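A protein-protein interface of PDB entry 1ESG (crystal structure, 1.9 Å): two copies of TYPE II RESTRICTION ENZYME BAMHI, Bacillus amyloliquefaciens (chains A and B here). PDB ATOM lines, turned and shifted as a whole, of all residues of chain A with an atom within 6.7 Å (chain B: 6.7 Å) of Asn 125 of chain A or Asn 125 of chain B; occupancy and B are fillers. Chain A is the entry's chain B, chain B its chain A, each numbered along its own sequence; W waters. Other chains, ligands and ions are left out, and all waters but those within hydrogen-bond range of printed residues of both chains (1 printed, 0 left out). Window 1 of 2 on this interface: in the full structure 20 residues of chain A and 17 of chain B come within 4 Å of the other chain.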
ATOM      1  N   ALA A 120     -17.748  32.728 -13.808  1.00  0.00           N
ATOM      2  CA  ALA A 120     -19.195  32.818 -13.585  1.00  0.00           C
ATOM      3  C   ALA A 120     -19.844  31.465 -13.860  1.00  0.00           C
ATOM      4  O   ALA A 120     -20.818  31.081 -13.212  1.00  0.00           O
ATOM      5  CB  ALA A 120     -19.803  33.889 -14.483  1.00  0.00           C
ATOM      6  N   HIS A 121     -19.308  30.745 -14.842  1.00  0.00           N
ATOM      7  CA  HIS A 121     -19.808  29.409 -15.133  1.00  0.00           C
ATOM      8  C   HIS A 121     -19.509  28.534 -13.920  1.00  0.00           C
ATOM      9  O   HIS A 121     -20.325  27.701 -13.542  1.00  0.00           O
ATOM     10  CB  HIS A 121     -19.100  28.809 -16.364  1.00  0.00           C
ATOM     11  CG  HIS A 121     -19.690  29.250 -17.662  1.00  0.00           C
ATOM     12  ND1 HIS A 121     -20.777  28.622 -18.234  1.00  0.00           N
ATOM     13  CD2 HIS A 121     -19.386  30.293 -18.471  1.00  0.00           C
ATOM     14  CE1 HIS A 121     -21.117  29.259 -19.341  1.00  0.00           C
ATOM     15  NE2 HIS A 121     -20.288  30.276 -19.508  1.00  0.00           N
ATOM     16  N   ARG A 122     -18.335  28.709 -13.317  1.00  0.00           N
ATOM     17  CA  ARG A 122     -17.978  27.878 -12.150  1.00  0.00           C
ATOM     18  C   ARG A 122     -18.903  28.203 -10.972  1.00  0.00           C
ATOM     19  O   ARG A 122     -19.359  27.305 -10.252  1.00  0.00           O
ATOM     20  CB  ARG A 122     -16.521  28.106 -11.732  1.00  0.00           C
ATOM     21  CG  ARG A 122     -16.109  27.175 -10.592  1.00  0.00           C
ATOM     22  CD  ARG A 122     -14.615  27.190 -10.333  1.00  0.00           C
ATOM     23  NE  ARG A 122     -14.213  28.366  -9.573  1.00  0.00           N
ATOM     24  CZ  ARG A 122     -13.175  28.397  -8.745  1.00  0.00           C
ATOM     25  NH1 ARG A 122     -12.430  27.312  -8.567  1.00  0.00           N
ATOM     26  NH2 ARG A 122     -12.884  29.513  -8.089  1.00  0.00           N
ATOM     27  N   SER A 123     -19.180  29.492 -10.789  1.00  0.00           N
ATOM     28  CA  SER A 123     -20.086  29.944  -9.713  1.00  0.00           C
ATOM     29  C   SER A 123     -21.503  29.371  -9.904  1.00  0.00           C
ATOM     30  O   SER A 123     -22.116  28.834  -8.967  1.00  0.00           O
ATOM     31  CB  SER A 123     -20.116  31.498  -9.698  1.00  0.00           C
ATOM     32  OG  SER A 123     -21.067  31.990  -8.753  1.00  0.00           O
ATOM     33  N   MET A 124     -22.041  29.484 -11.121  1.00  0.00           N
ATOM     34  CA  MET A 124     -23.371  28.937 -11.381  1.00  0.00           C
ATOM     35  C   MET A 124     -23.378  27.425 -11.095  1.00  0.00           C
ATOM     36  O   MET A 124     -24.337  26.897 -10.525  1.00  0.00           O
ATOM     37  CB  MET A 124     -23.772  29.181 -12.846  1.00  0.00           C
ATOM     38  CG  MET A 124     -25.147  28.628 -13.224  1.00  0.00           C
ATOM     39  SD  MET A 124     -25.621  29.076 -14.932  1.00  0.00           S
ATOM     40  CE  MET A 124     -24.613  27.919 -15.901  1.00  0.00           C
ATOM     41  N   ASN A 125     -22.323  26.718 -11.507  1.00  0.00           N
ATOM     42  CA  ASN A 125     -22.255  25.263 -11.273  1.00  0.00           C
ATOM     43  C   ASN A 125     -22.104  24.941  -9.776  1.00  0.00           C
ATOM     44  O   ASN A 125     -22.626  23.939  -9.287  1.00  0.00           O
ATOM     45  CB  ASN A 125     -21.094  24.635 -12.056  1.00  0.00           C
ATOM     46  CG  ASN A 125     -21.417  24.448 -13.551  1.00  0.00           C
ATOM     47  OD1 ASN A 125     -20.568  24.010 -14.338  1.00  0.00           O
ATOM     48  ND2 ASN A 125     -22.631  24.775 -13.935  1.00  0.00           N
ATOM     49  N   LYS A 126     -21.386  25.785  -9.050  1.00  0.00           N
ATOM     50  CA  LYS A 126     -21.236  25.560  -7.614  1.00  0.00           C
ATOM     51  C   LYS A 126     -22.624  25.630  -6.959  1.00  0.00           C
ATOM     52  O   LYS A 126     -22.992  24.785  -6.133  1.00  0.00           O
ATOM     53  CB  LYS A 126     -20.310  26.616  -7.006  1.00  0.00           C
ATOM     54  CG  LYS A 126     -20.183  26.512  -5.488  1.00  0.00           C
ATOM     55  CD  LYS A 126     -19.605  27.789  -4.852  1.00  0.00           C
ATOM     56  CE  LYS A 126     -18.240  28.170  -5.401  1.00  0.00           C
ATOM     57  NZ  LYS A 126     -17.704  29.370  -4.670  1.00  0.00           N
ATOM     58  N   LEU A 127     -23.395  26.637  -7.343  1.00  0.00           N
ATOM     59  CA  LEU A 127     -24.755  26.833  -6.818  1.00  0.00           C
ATOM     60  C   LEU A 127     -25.670  25.672  -7.247  1.00  0.00           C
ATOM     61  O   LEU A 127     -26.456  25.165  -6.454  1.00  0.00           O
ATOM     62  CB  LEU A 127     -25.306  28.171  -7.346  1.00  0.00           C
ATOM     63  CG  LEU A 127     -25.409  29.486  -6.549  1.00  0.00           C
ATOM     64  CD1 LEU A 127     -24.852  29.385  -5.157  1.00  0.00           C
ATOM     65  CD2 LEU A 127     -24.749  30.588  -7.343  1.00  0.00           C
ATOM     66  N   LEU A 128     -25.573  25.256  -8.506  1.00  0.00           N
ATOM     67  CA  LEU A 128     -26.377  24.141  -9.000  1.00  0.00           C
ATOM     68  C   LEU A 128     -26.099  22.834  -8.244  1.00  0.00           C
ATOM     69  O   LEU A 128     -27.015  22.068  -7.957  1.00  0.00           O
ATOM     70  CB  LEU A 128     -26.120  23.912 -10.490  1.00  0.00           C
ATOM     71  CG  LEU A 128     -26.803  24.867 -11.458  1.00  0.00           C
ATOM     72  CD1 LEU A 128     -26.348  24.558 -12.889  1.00  0.00           C
ATOM     73  CD2 LEU A 128     -28.316  24.715 -11.327  1.00  0.00           C
ATOM     74  N   LEU A 129     -24.833  22.572  -7.938  1.00  0.00           N
ATOM     75  CA  LEU A 129     -24.494  21.361  -7.200  1.00  0.00           C
ATOM     76  C   LEU A 129     -25.051  21.481  -5.770  1.00  0.00           C
ATOM     77  O   LEU A 129     -25.499  20.492  -5.181  1.00  0.00           O
ATOM     78  CB  LEU A 129     -22.973  21.173  -7.162  1.00  0.00           C
ATOM     79  CG  LEU A 129     -22.506  19.793  -6.678  1.00  0.00           C
ATOM     80  CD1 LEU A 129     -22.937  18.708  -7.673  1.00  0.00           C
ATOM     81  CD2 LEU A 129     -20.983  19.815  -6.537  1.00  0.00           C
ATOM     82  N   GLY A 130     -25.031  22.692  -5.226  1.00  0.00           N
ATOM     83  CA  GLY A 130     -25.565  22.909  -3.887  1.00  0.00           C
ATOM     84  C   GLY A 130     -27.051  22.629  -3.846  1.00  0.00           C
ATOM     85  O   GLY A 130     -27.572  22.069  -2.869  1.00  0.00           O
ATOM     86  N   ILE A 141     -27.706  34.678  -8.406  1.00  0.00           N
ATOM     87  CA  ILE A 141     -26.456  35.215  -8.916  1.00  0.00           C
ATOM     88  C   ILE A 141     -26.674  36.678  -9.315  1.00  0.00           C
ATOM     89  O   ILE A 141     -27.686  37.003  -9.934  1.00  0.00           O
ATOM     90  CB  ILE A 141     -25.948  34.440 -10.152  1.00  0.00           C
ATOM     91  CG1 ILE A 141     -25.209  33.166  -9.718  1.00  0.00           C
ATOM     92  CG2 ILE A 141     -25.033  35.331 -10.976  1.00  0.00           C
ATOM     93  CD1 ILE A 141     -24.706  32.307 -10.936  1.00  0.00           C
ATOM     94  N   LEU A 162     -23.734  35.692 -19.675  1.00  0.00           N
ATOM     95  CA  LEU A 162     -24.091  34.415 -19.086  1.00  0.00           C
ATOM     96  C   LEU A 162     -25.513  33.995 -19.485  1.00  0.00           C
ATOM     97  O   LEU A 162     -25.833  32.819 -19.450  1.00  0.00           O
ATOM     98  CB  LEU A 162     -23.984  34.472 -17.552  1.00  0.00           C
ATOM     99  CG  LEU A 162     -24.205  33.146 -16.814  1.00  0.00           C
ATOM    100  CD1 LEU A 162     -23.131  32.128 -17.271  1.00  0.00           C
ATOM    101  CD2 LEU A 162     -24.114  33.348 -15.284  1.00  0.00           C
ATOM    102  N   TYR A 165     -26.809  30.773 -21.143  1.00  0.00           N
ATOM    103  CA  TYR A 165     -26.684  29.583 -20.296  1.00  0.00           C
ATOM    104  C   TYR A 165     -27.674  29.482 -19.138  1.00  0.00           C
ATOM    105  O   TYR A 165     -27.666  28.495 -18.404  1.00  0.00           O
ATOM    106  CB  TYR A 165     -25.248  29.488 -19.762  1.00  0.00           C
ATOM    107  CG  TYR A 165     -24.258  29.217 -20.870  1.00  0.00           C
ATOM    108  CD1 TYR A 165     -23.990  27.910 -21.281  1.00  0.00           C
ATOM    109  CD2 TYR A 165     -23.662  30.269 -21.568  1.00  0.00           C
ATOM    110  CE1 TYR A 165     -23.159  27.651 -22.367  1.00  0.00           C
ATOM    111  CE2 TYR A 165     -22.825  30.026 -22.657  1.00  0.00           C
ATOM    112  CZ  TYR A 165     -22.582  28.711 -23.051  1.00  0.00           C
ATOM    113  OH  TYR A 165     -21.770  28.452 -24.133  1.00  0.00           O
ATOM    114  N   LEU A 168     -29.581  26.265 -18.492  1.00  0.00           N
ATOM    115  CA  LEU A 168     -29.006  25.080 -17.852  1.00  0.00           C
ATOM    116  C   LEU A 168     -29.519  24.982 -16.420  1.00  0.00           C
ATOM    117  O   LEU A 168     -29.306  23.960 -15.764  1.00  0.00           O
ATOM    118  CB  LEU A 168     -27.477  25.135 -17.836  1.00  0.00           C
ATOM    119  CG  LEU A 168     -26.814  25.156 -19.216  1.00  0.00           C
ATOM    120  CD1 LEU A 168     -25.299  24.979 -19.040  1.00  0.00           C
ATOM    121  CD2 LEU A 168     -27.363  24.031 -20.079  1.00  0.00           C
ATOM    122  N   PHE A 174     -33.612  28.986  -9.381  1.00  0.00           N
ATOM    123  CA  PHE A 174     -32.459  29.830  -9.622  1.00  0.00           C
ATOM    124  C   PHE A 174     -32.913  31.201 -10.086  1.00  0.00           C
ATOM    125  O   PHE A 174     -33.891  31.324 -10.808  1.00  0.00           O
ATOM    126  CB  PHE A 174     -31.590  29.158 -10.716  1.00  0.00           C
ATOM    127  CG  PHE A 174     -30.117  29.305 -10.493  1.00  0.00           C
ATOM    128  CD1 PHE A 174     -29.514  30.561 -10.520  1.00  0.00           C
ATOM    129  CD2 PHE A 174     -29.329  28.185 -10.248  1.00  0.00           C
ATOM    130  CE1 PHE A 174     -28.127  30.704 -10.302  1.00  0.00           C
ATOM    131  CE2 PHE A 174     -27.960  28.308 -10.029  1.00  0.00           C
ATOM    132  CZ  PHE A 174     -27.355  29.566 -10.056  1.00  0.00           C
ATOM    133  N   ALA B 120     -12.784  24.850 -17.486  1.00  0.00           N
ATOM    134  CA  ALA B 120     -13.356  23.502 -17.718  1.00  0.00           C
ATOM    135  C   ALA B 120     -14.862  23.540 -17.446  1.00  0.00           C
ATOM    136  O   ALA B 120     -15.643  22.846 -18.099  1.00  0.00           O
ATOM    137  CB  ALA B 120     -12.690  22.455 -16.814  1.00  0.00           C
ATOM    138  N   HIS B 121     -15.274  24.336 -16.458  1.00  0.00           N
ATOM    139  CA  HIS B 121     -16.694  24.459 -16.160  1.00  0.00           C
ATOM    140  C   HIS B 121     -17.367  25.110 -17.358  1.00  0.00           C
ATOM    141  O   HIS B 121     -18.477  24.722 -17.735  1.00  0.00           O
ATOM    142  CB  HIS B 121     -16.923  25.332 -14.911  1.00  0.00           C
ATOM    143  CG  HIS B 121     -16.747  24.597 -13.619  1.00  0.00           C
ATOM    144  ND1 HIS B 121     -17.769  23.896 -13.020  1.00  0.00           N
ATOM    145  CD2 HIS B 121     -15.657  24.419 -12.836  1.00  0.00           C
ATOM    146  CE1 HIS B 121     -17.317  23.312 -11.922  1.00  0.00           C
ATOM    147  NE2 HIS B 121     -16.037  23.615 -11.788  1.00  0.00           N
ATOM    148  N   ARG B 122     -16.706  26.100 -17.955  1.00  0.00           N
ATOM    149  CA  ARG B 122     -17.294  26.764 -19.120  1.00  0.00           C
ATOM    150  C   ARG B 122     -17.419  25.791 -20.277  1.00  0.00           C
ATOM    151  O   ARG B 122     -18.433  25.790 -21.003  1.00  0.00           O
ATOM    152  CB  ARG B 122     -16.461  27.977 -19.560  1.00  0.00           C
ATOM    153  CG  ARG B 122     -17.114  28.737 -20.737  1.00  0.00           C
ATOM    154  CD  ARG B 122     -16.368  30.021 -21.113  1.00  0.00           C
ATOM    155  NE  ARG B 122     -15.075  29.704 -21.701  1.00  0.00           N
ATOM    156  CZ  ARG B 122     -14.165  30.600 -22.069  1.00  0.00           C
ATOM    157  NH1 ARG B 122     -14.398  31.898 -21.918  1.00  0.00           N
ATOM    158  NH2 ARG B 122     -13.012  30.188 -22.581  1.00  0.00           N
ATOM    159  N   SER B 123     -16.382  24.974 -20.460  1.00  0.00           N
ATOM    160  CA  SER B 123     -16.361  23.966 -21.530  1.00  0.00           C
ATOM    161  C   SER B 123     -17.482  22.936 -21.341  1.00  0.00           C
ATOM    162  O   SER B 123     -18.204  22.605 -22.287  1.00  0.00           O
ATOM    163  CB  SER B 123     -14.977  23.272 -21.559  1.00  0.00           C
ATOM    164  OG  SER B 123     -14.960  22.144 -22.447  1.00  0.00           O
ATOM    165  N   MET B 124     -17.630  22.418 -20.124  1.00  0.00           N
ATOM    166  CA  MET B 124     -18.693  21.456 -19.854  1.00  0.00           C
ATOM    167  C   MET B 124     -20.068  22.069 -20.157  1.00  0.00           C
ATOM    168  O   MET B 124     -20.932  21.413 -20.747  1.00  0.00           O
ATOM    169  CB  MET B 124     -18.657  21.005 -18.381  1.00  0.00           C
ATOM    170  CG  MET B 124     -19.661  19.886 -18.044  1.00  0.00           C
ATOM    171  SD  MET B 124     -19.509  19.348 -16.308  1.00  0.00           S
ATOM    172  CE  MET B 124     -20.186  20.798 -15.428  1.00  0.00           C
ATOM    173  N   ASN B 125     -20.278  23.320 -19.741  1.00  0.00           N
ATOM    174  CA  ASN B 125     -21.556  23.998 -19.966  1.00  0.00           C
ATOM    175  C   ASN B 125     -21.796  24.282 -21.467  1.00  0.00           C
ATOM    176  O   ASN B 125     -22.929  24.265 -21.938  1.00  0.00           O
ATOM    177  CB  ASN B 125     -21.621  25.318 -19.162  1.00  0.00           C
ATOM    178  CG  ASN B 125     -21.835  25.094 -17.652  1.00  0.00           C
ATOM    179  OD1 ASN B 125     -21.824  26.052 -16.853  1.00  0.00           O
ATOM    180  ND2 ASN B 125     -22.022  23.854 -17.260  1.00  0.00           N
ATOM    181  N   LYS B 126     -20.729  24.558 -22.207  1.00  0.00           N
ATOM    182  CA  LYS B 126     -20.816  24.790 -23.657  1.00  0.00           C
ATOM    183  C   LYS B 126     -21.400  23.506 -24.270  1.00  0.00           C
ATOM    184  O   LYS B 126     -22.334  23.526 -25.076  1.00  0.00           O
ATOM    185  CB  LYS B 126     -19.412  24.934 -24.237  1.00  0.00           C
ATOM    186  CG  LYS B 126     -18.951  26.232 -24.814  1.00  0.00           C
ATOM    187  CD  LYS B 126     -17.872  25.863 -25.837  1.00  0.00           C
ATOM    188  CE  LYS B 126     -16.755  26.865 -25.939  1.00  0.00           C
ATOM    189  NZ  LYS B 126     -15.707  26.287 -26.810  1.00  0.00           N
ATOM    190  N   LEU B 127     -20.810  22.384 -23.884  1.00  0.00           N
ATOM    191  CA  LEU B 127     -21.238  21.077 -24.380  1.00  0.00           C
ATOM    192  C   LEU B 127     -22.658  20.730 -23.954  1.00  0.00           C
ATOM    193  O   LEU B 127     -23.432  20.197 -24.741  1.00  0.00           O
ATOM    194  CB  LEU B 127     -20.264  20.004 -23.892  1.00  0.00           C
ATOM    195  CG  LEU B 127     -18.918  20.045 -24.643  1.00  0.00           C
ATOM    196  CD1 LEU B 127     -17.900  19.222 -23.882  1.00  0.00           C
ATOM    197  CD2 LEU B 127     -19.081  19.490 -26.075  1.00  0.00           C
ATOM    198  N   LEU B 128     -22.990  21.010 -22.702  1.00  0.00           N
ATOM    199  CA  LEU B 128     -24.334  20.757 -22.200  1.00  0.00           C
ATOM    200  C   LEU B 128     -25.364  21.577 -22.964  1.00  0.00           C
ATOM    201  O   LEU B 128     -26.456  21.077 -23.284  1.00  0.00           O
ATOM    202  CB  LEU B 128     -24.431  21.101 -20.702  1.00  0.00           C
ATOM    203  CG  LEU B 128     -23.916  20.067 -19.705  1.00  0.00           C
ATOM    204  CD1 LEU B 128     -24.042  20.606 -18.262  1.00  0.00           C
ATOM    205  CD2 LEU B 128     -24.753  18.786 -19.858  1.00  0.00           C
ATOM    206  N   LEU B 129     -25.045  22.835 -23.262  1.00  0.00           N
ATOM    207  CA  LEU B 129     -25.999  23.664 -23.993  1.00  0.00           C
ATOM    208  C   LEU B 129     -26.158  23.113 -25.411  1.00  0.00           C
ATOM    209  O   LEU B 129     -27.252  23.146 -25.969  1.00  0.00           O
ATOM    210  CB  LEU B 129     -25.537  25.134 -24.047  1.00  0.00           C
ATOM    211  CG  LEU B 129     -26.572  26.157 -24.531  1.00  0.00           C
ATOM    212  CD1 LEU B 129     -27.741  26.226 -23.533  1.00  0.00           C
ATOM    213  CD2 LEU B 129     -25.925  27.543 -24.663  1.00  0.00           C
ATOM    214  N   GLY B 130     -25.075  22.578 -25.975  1.00  0.00           N
ATOM    215  CA  GLY B 130     -25.142  22.012 -27.328  1.00  0.00           C
ATOM    216  C   GLY B 130     -26.024  20.779 -27.367  1.00  0.00           C
ATOM    217  O   GLY B 130     -26.753  20.535 -28.328  1.00  0.00           O
ATOM    218  N   ILE B 141     -15.351  15.070 -22.845  1.00  0.00           N
ATOM    219  CA  ILE B 141     -14.326  15.958 -22.324  1.00  0.00           C
ATOM    220  C   ILE B 141     -13.116  15.119 -21.933  1.00  0.00           C
ATOM    221  O   ILE B 141     -13.263  14.074 -21.302  1.00  0.00           O
ATOM    222  CB  ILE B 141     -14.829  16.733 -21.067  1.00  0.00           C
ATOM    223  CG1 ILE B 141     -15.663  17.944 -21.504  1.00  0.00           C
ATOM    224  CG2 ILE B 141     -13.639  17.161 -20.193  1.00  0.00           C
ATOM    225  CD1 ILE B 141     -16.215  18.778 -20.307  1.00  0.00           C
ATOM    226  N   LEU B 162     -12.658  18.180 -11.550  1.00  0.00           N
ATOM    227  CA  LEU B 162     -13.972  18.410 -12.129  1.00  0.00           C
ATOM    228  C   LEU B 162     -14.982  17.323 -11.723  1.00  0.00           C
ATOM    229  O   LEU B 162     -16.181  17.568 -11.725  1.00  0.00           O
ATOM    230  CB  LEU B 162     -13.887  18.468 -13.667  1.00  0.00           C
ATOM    231  CG  LEU B 162     -15.164  18.880 -14.418  1.00  0.00           C
ATOM    232  CD1 LEU B 162     -15.604  20.275 -13.928  1.00  0.00           C
ATOM    233  CD2 LEU B 162     -14.930  18.906 -15.947  1.00  0.00           C
ATOM    234  N   TYR B 165     -18.414  17.542 -10.092  1.00  0.00           N
ATOM    235  CA  TYR B 165     -19.441  18.173 -10.923  1.00  0.00           C
ATOM    236  C   TYR B 165     -19.964  17.314 -12.064  1.00  0.00           C
ATOM    237  O   TYR B 165     -20.852  17.738 -12.797  1.00  0.00           O
ATOM    238  CB  TYR B 165     -18.897  19.501 -11.483  1.00  0.00           C
ATOM    239  CG  TYR B 165     -18.696  20.519 -10.374  1.00  0.00           C
ATOM    240  CD1 TYR B 165     -19.760  21.294  -9.921  1.00  0.00           C
ATOM    241  CD2 TYR B 165     -17.467  20.634  -9.720  1.00  0.00           C
ATOM    242  CE1 TYR B 165     -19.608  22.164  -8.830  1.00  0.00           C
ATOM    243  CE2 TYR B 165     -17.300  21.492  -8.633  1.00  0.00           C
ATOM    244  CZ  TYR B 165     -18.377  22.253  -8.195  1.00  0.00           C
ATOM    245  OH  TYR B 165     -18.227  23.086  -7.108  1.00  0.00           O
ATOM    246  N   LEU B 168     -23.661  17.011 -12.706  1.00  0.00           N
ATOM    247  CA  LEU B 168     -24.473  18.050 -13.323  1.00  0.00           C
ATOM    248  C   LEU B 168     -24.800  17.628 -14.755  1.00  0.00           C
ATOM    249  O   LEU B 168     -25.614  18.261 -15.416  1.00  0.00           O
ATOM    250  CB  LEU B 168     -23.739  19.398 -13.330  1.00  0.00           C
ATOM    251  CG  LEU B 168     -23.520  20.014 -11.933  1.00  0.00           C
ATOM    252  CD1 LEU B 168     -23.020  21.442 -12.087  1.00  0.00           C
ATOM    253  CD2 LEU B 168     -24.832  20.015 -11.142  1.00  0.00           C
ATOM    254  N   PHE B 174     -23.086  12.119 -21.763  1.00  0.00           N
ATOM    255  CA  PHE B 174     -21.823  12.809 -21.565  1.00  0.00           C
ATOM    256  C   PHE B 174     -20.772  11.809 -21.102  1.00  0.00           C
ATOM    257  O   PHE B 174     -21.073  10.880 -20.353  1.00  0.00           O
ATOM    258  CB  PHE B 174     -22.022  13.909 -20.487  1.00  0.00           C
ATOM    259  CG  PHE B 174     -21.235  15.160 -20.740  1.00  0.00           C
ATOM    260  CD1 PHE B 174     -19.842  15.143 -20.700  1.00  0.00           C
ATOM    261  CD2 PHE B 174     -21.889  16.368 -20.972  1.00  0.00           C
ATOM    262  CE1 PHE B 174     -19.100  16.316 -20.877  1.00  0.00           C
ATOM    263  CE2 PHE B 174     -21.160  17.545 -21.149  1.00  0.00           C
ATOM    264  CZ  PHE B 174     -19.764  17.520 -21.099  1.00  0.00           C
HETATM  265  O   HOH W   1     -24.236  23.113 -15.583  1.00  0.00           O
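Of the 16 printed residues of chain A, 8 touch a printed residue of chain B.
Along chain A the printed residues that touch a printed residue of chain B span positions 121 to 168.
Of the 16 printed residues of chain B, 8 touch a printed residue of chain A.
Printed residues of chain B that touch a printed residue of chain A: His 121, Arg 122, Met 124, Asn 125, Lys 126, Leu 129, Tyr 165 and Leu 168.
Hydrophobic or aromatic side chains of chain B that line the printed part of chain A: His 121, Met 124, Leu 129, Tyr 165 and Leu 168.
Along chain B the printed residues that touch a printed residue of chain A span positions 121 to 168.
Ala 120 of chain A touches none of the printed residues of chain B.
Printed residues of chain B within 4 Å of Arg 122 of chain A: His 121.
Ser 123 of chain A touches none of the printed residues of chain B.
Of the printed residues of chain B, Asn 125 of chain A touches His 121, Met 124, Asn 125, Tyr 165 and Leu 168.
Asn 125 of chain B touches just these residues of chain A: His 121 (3.1 Å), Met 124 (3.5 Å), Asn 125 (3.3 Å), Tyr 165 (3.4 Å) and Leu 168 (3.7 Å).
Of the printed residues of chain A, Tyr 165 of chain B touches Asn 125, Lys 126 and Leu 129.
The nearest residue of chain B that does not touch Asn 125 of chain A is Arg 122 of chain B (5.7 Å).
The nearest residue of chain A that does not touch Asn 125 of chain B is Arg 122 of chain A (5.6 Å).
His 121 of chain A touches Arg 122 of chain B, and with the chains exchanged Arg 122 of chain A touches His 121 of chain B.
Asn 125 of chain A touches Leu 168 of chain B, and with the chains exchanged Leu 168 of chain A touches Asn 125 of chain B.
Lys 126 of chain A touches Tyr 165 of chain B, and with the chains exchanged Tyr 165 of chain A touches Lys 126 of chain B.
Leu 129 of chain A touches Tyr 165 of chain B, and with the chains exchanged Tyr 165 of chain A touches Leu 129 of chain B.
Positions printed for both chains: 120, 121, 122, 123, 124, 125, 126, 127, 128, 129, 130, 141, 162, 165, 168 and 174.
Of the 15 pairs that touch across the chains among the printed residues, 15 have their exchanged pair printed and touching as well.
Water W1 lies within hydrogen-bond range of the side-chain amide nitrogen (ND2) of Asn 125 of chain A (2.8 Å) and the side-chain amide nitrogen (ND2) of Asn 125 of chain B (2.9 Å).
Among the printed residues, merely in contact across the chains: His 121 of chain A with Arg 122 of chain B (3.6 Å), Arg 122 of chain A with His 121 of chain B (3.6 Å), Met 124 of chain A with Asn 125 of chain B (3.5 Å), Asn 125 of chain A with Met 124 of chain B (3.4 Å), Asn 125 of chain A with Tyr 165 of chain B (3.5 Å), Asn 125 of chain A with Leu 168 of chain B (3.7 Å), Lys 126 of chain A with Tyr 165 of chain B (3.9 Å), Leu 129 of chain A with Tyr 165 of chain B (3.6 Å), Tyr 165 of chain A with Asn 125 of chain B (3.4 Å), Tyr 165 of chain A with Lys 126 of chain B (3.7 Å), Tyr 165 of chain A with Leu 129 of chain B (3.6 Å) and Leu 168 of chain A with Asn 125 of chain B (3.7 Å).
OD1 of Asn 125 of chain B lies within hydrogen-bond range of ND1 of His 121 of chain A (3.1 Å).
A ring nitrogen (ND1) of His 121 of chain B sits at hydrogen-bond distance from the side-chain amide oxygen (OD1) of Asn 125 of chain A, 3.1 Å away.
The side-chain amide oxygen (OD1) of Asn 125 of chain A is in hydrogen-bond range of the side-chain amide nitrogen (ND2) of Asn 125 of chain B (3.3 Å).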
